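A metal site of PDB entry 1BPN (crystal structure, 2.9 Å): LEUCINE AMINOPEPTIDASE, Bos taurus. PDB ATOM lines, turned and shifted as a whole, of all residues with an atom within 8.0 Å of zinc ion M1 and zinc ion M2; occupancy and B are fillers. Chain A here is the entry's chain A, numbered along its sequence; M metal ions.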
ATOM      1  N   VAL A 219     -18.370  21.411 -29.420  1.00  0.00           N
ATOM      2  CA  VAL A 219     -17.265  20.599 -29.038  1.00  0.00           C
ATOM      3  C   VAL A 219     -17.680  19.576 -28.002  1.00  0.00           C
ATOM      4  O   VAL A 219     -17.341  18.407 -28.146  1.00  0.00           O
ATOM      5  CB  VAL A 219     -16.173  21.491 -28.495  1.00  0.00           C
ATOM      6  CG1 VAL A 219     -14.929  20.626 -28.331  1.00  0.00           C
ATOM      7  CG2 VAL A 219     -15.862  22.644 -29.433  1.00  0.00           C
ATOM      8  N   LYS A 250      -8.404  26.932 -21.771  1.00  0.00           N
ATOM      9  CA  LYS A 250      -9.067  25.796 -22.371  1.00  0.00           C
ATOM     10  C   LYS A 250      -8.939  24.542 -21.516  1.00  0.00           C
ATOM     11  O   LYS A 250      -7.889  24.191 -20.975  1.00  0.00           O
ATOM     12  CB  LYS A 250      -8.493  25.669 -23.797  1.00  0.00           C
ATOM     13  CG  LYS A 250      -7.326  24.778 -24.174  1.00  0.00           C
ATOM     14  CD  LYS A 250      -7.755  23.838 -25.264  1.00  0.00           C
ATOM     15  CE  LYS A 250      -6.555  23.496 -26.080  1.00  0.00           C
ATOM     16  NZ  LYS A 250      -6.685  22.151 -26.544  1.00  0.00           N
ATOM     17  N   GLY A 251     -10.093  23.905 -21.341  1.00  0.00           N
ATOM     18  CA  GLY A 251     -10.199  22.759 -20.468  1.00  0.00           C
ATOM     19  C   GLY A 251     -10.775  21.502 -21.098  1.00  0.00           C
ATOM     20  O   GLY A 251     -11.829  21.011 -20.675  1.00  0.00           O
ATOM     21  N   ILE A 252     -10.091  20.949 -22.098  1.00  0.00           N
ATOM     22  CA  ILE A 252     -10.508  19.660 -22.673  1.00  0.00           C
ATOM     23  C   ILE A 252      -9.950  18.627 -21.682  1.00  0.00           C
ATOM     24  O   ILE A 252      -8.712  18.539 -21.553  1.00  0.00           O
ATOM     25  CB  ILE A 252      -9.906  19.510 -24.090  1.00  0.00           C
ATOM     26  CG1 ILE A 252     -10.337  20.641 -25.045  1.00  0.00           C
ATOM     27  CG2 ILE A 252     -10.319  18.158 -24.600  1.00  0.00           C
ATOM     28  CD1 ILE A 252     -11.830  20.913 -25.372  1.00  0.00           C
ATOM     29  N   PHE A 254      -9.916  15.420 -21.774  1.00  0.00           N
ATOM     30  CA  PHE A 254      -9.259  14.523 -22.660  1.00  0.00           C
ATOM     31  C   PHE A 254      -9.571  14.911 -24.095  1.00  0.00           C
ATOM     32  O   PHE A 254     -10.748  15.101 -24.396  1.00  0.00           O
ATOM     33  CB  PHE A 254      -9.711  13.108 -22.430  1.00  0.00           C
ATOM     34  CG  PHE A 254      -8.736  12.191 -23.151  1.00  0.00           C
ATOM     35  CD1 PHE A 254      -7.489  11.991 -22.611  1.00  0.00           C
ATOM     36  CD2 PHE A 254      -9.055  11.702 -24.393  1.00  0.00           C
ATOM     37  CE1 PHE A 254      -6.519  11.391 -23.364  1.00  0.00           C
ATOM     38  CE2 PHE A 254      -8.084  11.067 -25.142  1.00  0.00           C
ATOM     39  CZ  PHE A 254      -6.808  10.929 -24.634  1.00  0.00           C
ATOM     40  N   ASP A 255      -8.486  15.040 -24.892  1.00  0.00           N
ATOM     41  CA  ASP A 255      -8.535  15.270 -26.353  1.00  0.00           C
ATOM     42  C   ASP A 255      -8.162  14.048 -27.224  1.00  0.00           C
ATOM     43  O   ASP A 255      -7.004  13.693 -27.385  1.00  0.00           O
ATOM     44  CB  ASP A 255      -7.601  16.401 -26.786  1.00  0.00           C
ATOM     45  CG  ASP A 255      -7.964  17.066 -28.133  1.00  0.00           C
ATOM     46  OD1 ASP A 255      -8.735  16.508 -28.941  1.00  0.00           O
ATOM     47  OD2 ASP A 255      -7.524  18.205 -28.362  1.00  0.00           O
ATOM     48  N   SER A 256      -9.108  13.361 -27.836  1.00  0.00           N
ATOM     49  CA  SER A 256      -8.838  12.269 -28.764  1.00  0.00           C
ATOM     50  C   SER A 256      -8.842  12.758 -30.230  1.00  0.00           C
ATOM     51  O   SER A 256      -8.767  11.971 -31.177  1.00  0.00           O
ATOM     52  CB  SER A 256      -9.908  11.219 -28.619  1.00  0.00           C
ATOM     53  OG  SER A 256     -11.177  11.665 -29.119  1.00  0.00           O
ATOM     54  N   GLY A 257      -9.060  14.070 -30.412  1.00  0.00           N
ATOM     55  CA  GLY A 257      -9.163  14.644 -31.731  1.00  0.00           C
ATOM     56  C   GLY A 257     -10.569  14.635 -32.261  1.00  0.00           C
ATOM     57  O   GLY A 257     -10.867  15.456 -33.125  1.00  0.00           O
ATOM     58  N   GLY A 258     -11.428  13.736 -31.762  1.00  0.00           N
ATOM     59  CA  GLY A 258     -12.796  13.587 -32.226  1.00  0.00           C
ATOM     60  C   GLY A 258     -12.875  12.744 -33.493  1.00  0.00           C
ATOM     61  O   GLY A 258     -12.241  11.694 -33.571  1.00  0.00           O
ATOM     62  N   SER A 260     -11.910  14.007 -36.349  1.00  0.00           N
ATOM     63  CA  SER A 260     -10.581  14.269 -36.875  1.00  0.00           C
ATOM     64  C   SER A 260      -9.545  13.837 -35.826  1.00  0.00           C
ATOM     65  O   SER A 260      -8.681  14.610 -35.414  1.00  0.00           O
ATOM     66  CB  SER A 260     -10.503  15.753 -37.247  1.00  0.00           C
ATOM     67  OG  SER A 260     -11.178  15.995 -38.488  1.00  0.00           O
ATOM     68  N   LYS A 262      -7.028  11.620 -33.459  1.00  0.00           N
ATOM     69  CA  LYS A 262      -5.626  11.450 -33.188  1.00  0.00           C
ATOM     70  C   LYS A 262      -5.106  10.039 -33.397  1.00  0.00           C
ATOM     71  O   LYS A 262      -5.838   9.064 -33.447  1.00  0.00           O
ATOM     72  CB  LYS A 262      -5.315  11.899 -31.743  1.00  0.00           C
ATOM     73  CG  LYS A 262      -5.647  13.372 -31.452  1.00  0.00           C
ATOM     74  CD  LYS A 262      -5.192  13.748 -30.057  1.00  0.00           C
ATOM     75  CE  LYS A 262      -5.292  15.251 -29.768  1.00  0.00           C
ATOM     76  NZ  LYS A 262      -4.487  16.034 -30.692  1.00  0.00           N
ATOM     77  N   MET A 270      -3.123  13.595 -23.591  1.00  0.00           N
ATOM     78  CA  MET A 270      -4.163  14.567 -23.944  1.00  0.00           C
ATOM     79  C   MET A 270      -5.076  14.925 -22.820  1.00  0.00           C
ATOM     80  O   MET A 270      -5.791  15.917 -22.897  1.00  0.00           O
ATOM     81  CB  MET A 270      -4.982  14.086 -25.108  1.00  0.00           C
ATOM     82  CG  MET A 270      -4.184  14.074 -26.391  1.00  0.00           C
ATOM     83  SD  MET A 270      -2.925  15.373 -26.631  1.00  0.00           S
ATOM     84  CE  MET A 270      -3.799  16.916 -26.590  1.00  0.00           C
ATOM     85  N   ALA A 272      -3.893  16.230 -20.516  1.00  0.00           N
ATOM     86  CA  ALA A 272      -3.399  17.506 -20.085  1.00  0.00           C
ATOM     87  C   ALA A 272      -3.663  18.578 -21.109  1.00  0.00           C
ATOM     88  O   ALA A 272      -2.929  19.562 -21.212  1.00  0.00           O
ATOM     89  CB  ALA A 272      -1.929  17.453 -19.838  1.00  0.00           C
ATOM     90  N   ASP A 273      -4.757  18.388 -21.877  1.00  0.00           N
ATOM     91  CA  ASP A 273      -5.227  19.424 -22.799  1.00  0.00           C
ATOM     92  C   ASP A 273      -6.167  20.368 -22.058  1.00  0.00           C
ATOM     93  O   ASP A 273      -6.659  21.346 -22.624  1.00  0.00           O
ATOM     94  CB  ASP A 273      -5.910  18.741 -23.967  1.00  0.00           C
ATOM     95  CG  ASP A 273      -5.988  19.610 -25.206  1.00  0.00           C
ATOM     96  OD1 ASP A 273      -5.001  20.262 -25.548  1.00  0.00           O
ATOM     97  OD2 ASP A 273      -7.048  19.626 -25.821  1.00  0.00           O
ATOM     98  N   MET A 274      -6.438  20.060 -20.766  1.00  0.00           N
ATOM     99  CA  MET A 274      -7.062  20.952 -19.785  1.00  0.00           C
ATOM    100  C   MET A 274      -5.995  21.759 -19.030  1.00  0.00           C
ATOM    101  O   MET A 274      -6.288  22.364 -17.997  1.00  0.00           O
ATOM    102  CB  MET A 274      -7.878  20.213 -18.723  1.00  0.00           C
ATOM    103  CG  MET A 274      -7.250  18.975 -18.103  1.00  0.00           C
ATOM    104  SD  MET A 274      -5.630  19.094 -17.309  1.00  0.00           S
ATOM    105  CE  MET A 274      -6.464  20.086 -16.095  1.00  0.00           C
ATOM    106  N   ASN A 305     -13.250  16.003 -25.904  1.00  0.00           N
ATOM    107  CA  ASN A 305     -13.367  15.866 -27.358  1.00  0.00           C
ATOM    108  C   ASN A 305     -13.281  14.395 -27.790  1.00  0.00           C
ATOM    109  O   ASN A 305     -12.244  13.736 -27.798  1.00  0.00           O
ATOM    110  CB  ASN A 305     -12.286  16.746 -27.973  1.00  0.00           C
ATOM    111  CG  ASN A 305     -12.500  16.995 -29.456  1.00  0.00           C
ATOM    112  OD1 ASN A 305     -11.531  16.995 -30.195  1.00  0.00           O
ATOM    113  ND2 ASN A 305     -13.729  17.168 -29.944  1.00  0.00           N
ATOM    114  N   ASN A 330     -11.612  20.676 -39.026  1.00  0.00           N
ATOM    115  CA  ASN A 330     -10.850  19.732 -38.260  1.00  0.00           C
ATOM    116  C   ASN A 330     -11.301  19.890 -36.824  1.00  0.00           C
ATOM    117  O   ASN A 330     -11.098  20.912 -36.175  1.00  0.00           O
ATOM    118  CB  ASN A 330      -9.370  20.037 -38.433  1.00  0.00           C
ATOM    119  CG  ASN A 330      -8.452  19.020 -37.775  1.00  0.00           C
ATOM    120  OD1 ASN A 330      -8.517  18.863 -36.568  1.00  0.00           O
ATOM    121  ND2 ASN A 330      -7.594  18.292 -38.498  1.00  0.00           N
ATOM    122  N   THR A 331     -11.879  18.774 -36.357  1.00  0.00           N
ATOM    123  CA  THR A 331     -12.437  18.544 -35.020  1.00  0.00           C
ATOM    124  C   THR A 331     -11.364  18.536 -33.914  1.00  0.00           C
ATOM    125  O   THR A 331     -11.662  18.640 -32.729  1.00  0.00           O
ATOM    126  CB  THR A 331     -13.245  17.207 -35.197  1.00  0.00           C
ATOM    127  OG1 THR A 331     -14.293  17.562 -36.088  1.00  0.00           O
ATOM    128  CG2 THR A 331     -13.999  16.633 -34.011  1.00  0.00           C
ATOM    129  N   ASP A 332     -10.056  18.435 -34.236  1.00  0.00           N
ATOM    130  CA  ASP A 332      -8.973  18.553 -33.270  1.00  0.00           C
ATOM    131  C   ASP A 332      -8.639  20.027 -33.072  1.00  0.00           C
ATOM    132  O   ASP A 332      -8.084  20.484 -32.078  1.00  0.00           O
ATOM    133  CB  ASP A 332      -7.784  17.778 -33.826  1.00  0.00           C
ATOM    134  CG  ASP A 332      -6.857  17.052 -32.861  1.00  0.00           C
ATOM    135  OD1 ASP A 332      -7.111  17.092 -31.661  1.00  0.00           O
ATOM    136  OD2 ASP A 332      -5.895  16.448 -33.313  1.00  0.00           O
ATOM    137  N   ALA A 333      -8.969  20.924 -33.990  1.00  0.00           N
ATOM    138  CA  ALA A 333      -8.837  22.341 -33.719  1.00  0.00           C
ATOM    139  C   ALA A 333     -10.036  22.763 -32.805  1.00  0.00           C
ATOM    140  O   ALA A 333     -10.840  23.609 -33.188  1.00  0.00           O
ATOM    141  CB  ALA A 333      -8.851  23.013 -35.085  1.00  0.00           C
ATOM    142  N   GLU A 334     -10.244  22.217 -31.599  1.00  0.00           N
ATOM    143  CA  GLU A 334     -11.407  22.527 -30.759  1.00  0.00           C
ATOM    144  C   GLU A 334     -11.187  23.477 -29.591  1.00  0.00           C
ATOM    145  O   GLU A 334     -12.113  24.032 -29.020  1.00  0.00           O
ATOM    146  CB  GLU A 334     -11.979  21.224 -30.223  1.00  0.00           C
ATOM    147  CG  GLU A 334     -11.379  20.566 -28.986  1.00  0.00           C
ATOM    148  CD  GLU A 334      -9.870  20.316 -29.085  1.00  0.00           C
ATOM    149  OE1 GLU A 334      -9.461  19.492 -29.938  1.00  0.00           O
ATOM    150  OE2 GLU A 334      -9.115  20.933 -28.323  1.00  0.00           O
ATOM    151  N   GLY A 335      -9.945  23.626 -29.181  1.00  0.00           N
ATOM    152  CA  GLY A 335      -9.566  24.562 -28.155  1.00  0.00           C
ATOM    153  C   GLY A 335      -9.848  25.928 -28.683  1.00  0.00           C
ATOM    154  O   GLY A 335     -10.444  26.673 -27.948  1.00  0.00           O
ATOM    155  N   ARG A 336      -9.509  26.223 -29.958  1.00  0.00           N
ATOM    156  CA  ARG A 336      -9.848  27.482 -30.620  1.00  0.00           C
ATOM    157  C   ARG A 336     -11.359  27.777 -30.468  1.00  0.00           C
ATOM    158  O   ARG A 336     -11.779  28.915 -30.204  1.00  0.00           O
ATOM    159  CB  ARG A 336      -9.560  27.478 -32.157  1.00  0.00           C
ATOM    160  CG  ARG A 336      -8.919  26.312 -32.930  1.00  0.00           C
ATOM    161  CD  ARG A 336      -7.370  26.326 -32.963  1.00  0.00           C
ATOM    162  NE  ARG A 336      -6.594  25.055 -32.799  1.00  0.00           N
ATOM    163  CZ  ARG A 336      -6.661  24.156 -31.766  1.00  0.00           C
ATOM    164  NH1 ARG A 336      -7.514  24.164 -30.752  1.00  0.00           N
ATOM    165  NH2 ARG A 336      -5.851  23.114 -31.761  1.00  0.00           N
ATOM    166  N   ILE A 338     -13.560  26.355 -28.185  1.00  0.00           N
ATOM    167  CA  ILE A 338     -13.936  26.338 -26.778  1.00  0.00           C
ATOM    168  C   ILE A 338     -13.643  27.749 -26.254  1.00  0.00           C
ATOM    169  O   ILE A 338     -14.489  28.335 -25.569  1.00  0.00           O
ATOM    170  CB  ILE A 338     -13.097  25.139 -26.116  1.00  0.00           C
ATOM    171  CG1 ILE A 338     -14.015  24.472 -25.186  1.00  0.00           C
ATOM    172  CG2 ILE A 338     -11.949  25.485 -25.198  1.00  0.00           C
ATOM    173  CD1 ILE A 338     -14.943  23.611 -26.002  1.00  0.00           C
ATOM    174  N   ALA A 358      -3.618  28.208 -23.177  1.00  0.00           N
ATOM    175  CA  ALA A 358      -4.094  26.986 -23.717  1.00  0.00           C
ATOM    176  C   ALA A 358      -3.024  26.149 -24.317  1.00  0.00           C
ATOM    177  O   ALA A 358      -2.181  26.655 -25.037  1.00  0.00           O
ATOM    178  CB  ALA A 358      -5.123  27.270 -24.790  1.00  0.00           C
ATOM    179  N   THR A 359      -3.143  24.843 -24.075  1.00  0.00           N
ATOM    180  CA  THR A 359      -2.331  23.820 -24.737  1.00  0.00           C
ATOM    181  C   THR A 359      -2.931  23.744 -26.143  1.00  0.00           C
ATOM    182  O   THR A 359      -3.562  22.746 -26.513  1.00  0.00           O
ATOM    183  CB  THR A 359      -2.492  22.518 -23.936  1.00  0.00           C
ATOM    184  OG1 THR A 359      -3.900  22.365 -23.743  1.00  0.00           O
ATOM    185  CG2 THR A 359      -1.770  22.522 -22.617  1.00  0.00           C
ATOM    186  N   LEU A 360      -2.785  24.818 -26.927  1.00  0.00           N
ATOM    187  CA  LEU A 360      -3.504  24.935 -28.163  1.00  0.00           C
ATOM    188  C   LEU A 360      -3.041  24.182 -29.397  1.00  0.00           C
ATOM    189  O   LEU A 360      -3.888  23.579 -30.057  1.00  0.00           O
ATOM    190  CB  LEU A 360      -3.626  26.389 -28.578  1.00  0.00           C
ATOM    191  CG  LEU A 360      -4.954  27.166 -28.668  1.00  0.00           C
ATOM    192  CD1 LEU A 360      -4.792  28.186 -29.778  1.00  0.00           C
ATOM    193  CD2 LEU A 360      -6.119  26.314 -29.079  1.00  0.00           C
ATOM    194  N   THR A 361      -1.742  24.166 -29.755  1.00  0.00           N
ATOM    195  CA  THR A 361      -1.226  23.583 -30.998  1.00  0.00           C
ATOM    196  C   THR A 361       0.115  22.914 -30.749  1.00  0.00           C
ATOM    197  O   THR A 361       0.986  23.413 -30.046  1.00  0.00           O
ATOM    198  CB  THR A 361      -0.979  24.674 -32.142  1.00  0.00           C
ATOM    199  OG1 THR A 361       0.056  25.567 -31.695  1.00  0.00           O
ATOM    200  CG2 THR A 361      -2.185  25.518 -32.459  1.00  0.00           C
HETATM  201 ZN    ZN M   1      -7.383  18.935 -30.447  1.00  0.00          ZN
HETATM  202 ZN    ZN M   2      -7.081  20.317 -27.866  1.00  0.00          ZN
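The backbone carbonyl oxygen (O) of Asp 273 sits at hydrogen-bond distance from the backbone NH (N) of Ile 252 (3.5 Å).
The side-chain carboxylate (OD1) of Asp 255 lies close to the side-chain amide oxygen (OD1) of Asn 305, 3.1 Å away.
N of Asp 255 sits at hydrogen-bond distance from O of Met 270, 3.5 Å away.
The side-chain carboxylate (OD2) of Asp 332 is in salt-bridge range of the side-chain amino group (NZ) of Lys 262, at 3.0 Å.
O of Asp 332 lies close to NH2 of Arg 336.
O of Gly 257 lies within hydrogen-bond range of N of Asp 332.
The side-chain amide oxygen of Asn 330 lies within hydrogen-bond range of the backbone NH of Asp 332, 2.8 Å away.
The side-chain amino group of Lys 250 lies close to the backbone carbonyl oxygen of Thr 359 (3.2 Å).
Of the 28 residues printed, 3 come within 4 Å of zinc ion M1.
Of the 28 residues printed, 4 come within 4 Å of zinc ion M2.
Zinc ion M1 is bound by OE1 of Glu 334, OD2 of Asp 255, OD1 of Asp 332 and O of Asp 332.
Zinc ion M1 has four donor atoms within binding distance.
Zinc ion M2 is bound by OD2 of Asp 273 (2.2 Å), OE2 of Glu 334 (2.2 Å), OD2 of Asp 255 (2.2 Å) and NZ of Lys 250 (2.3 Å).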
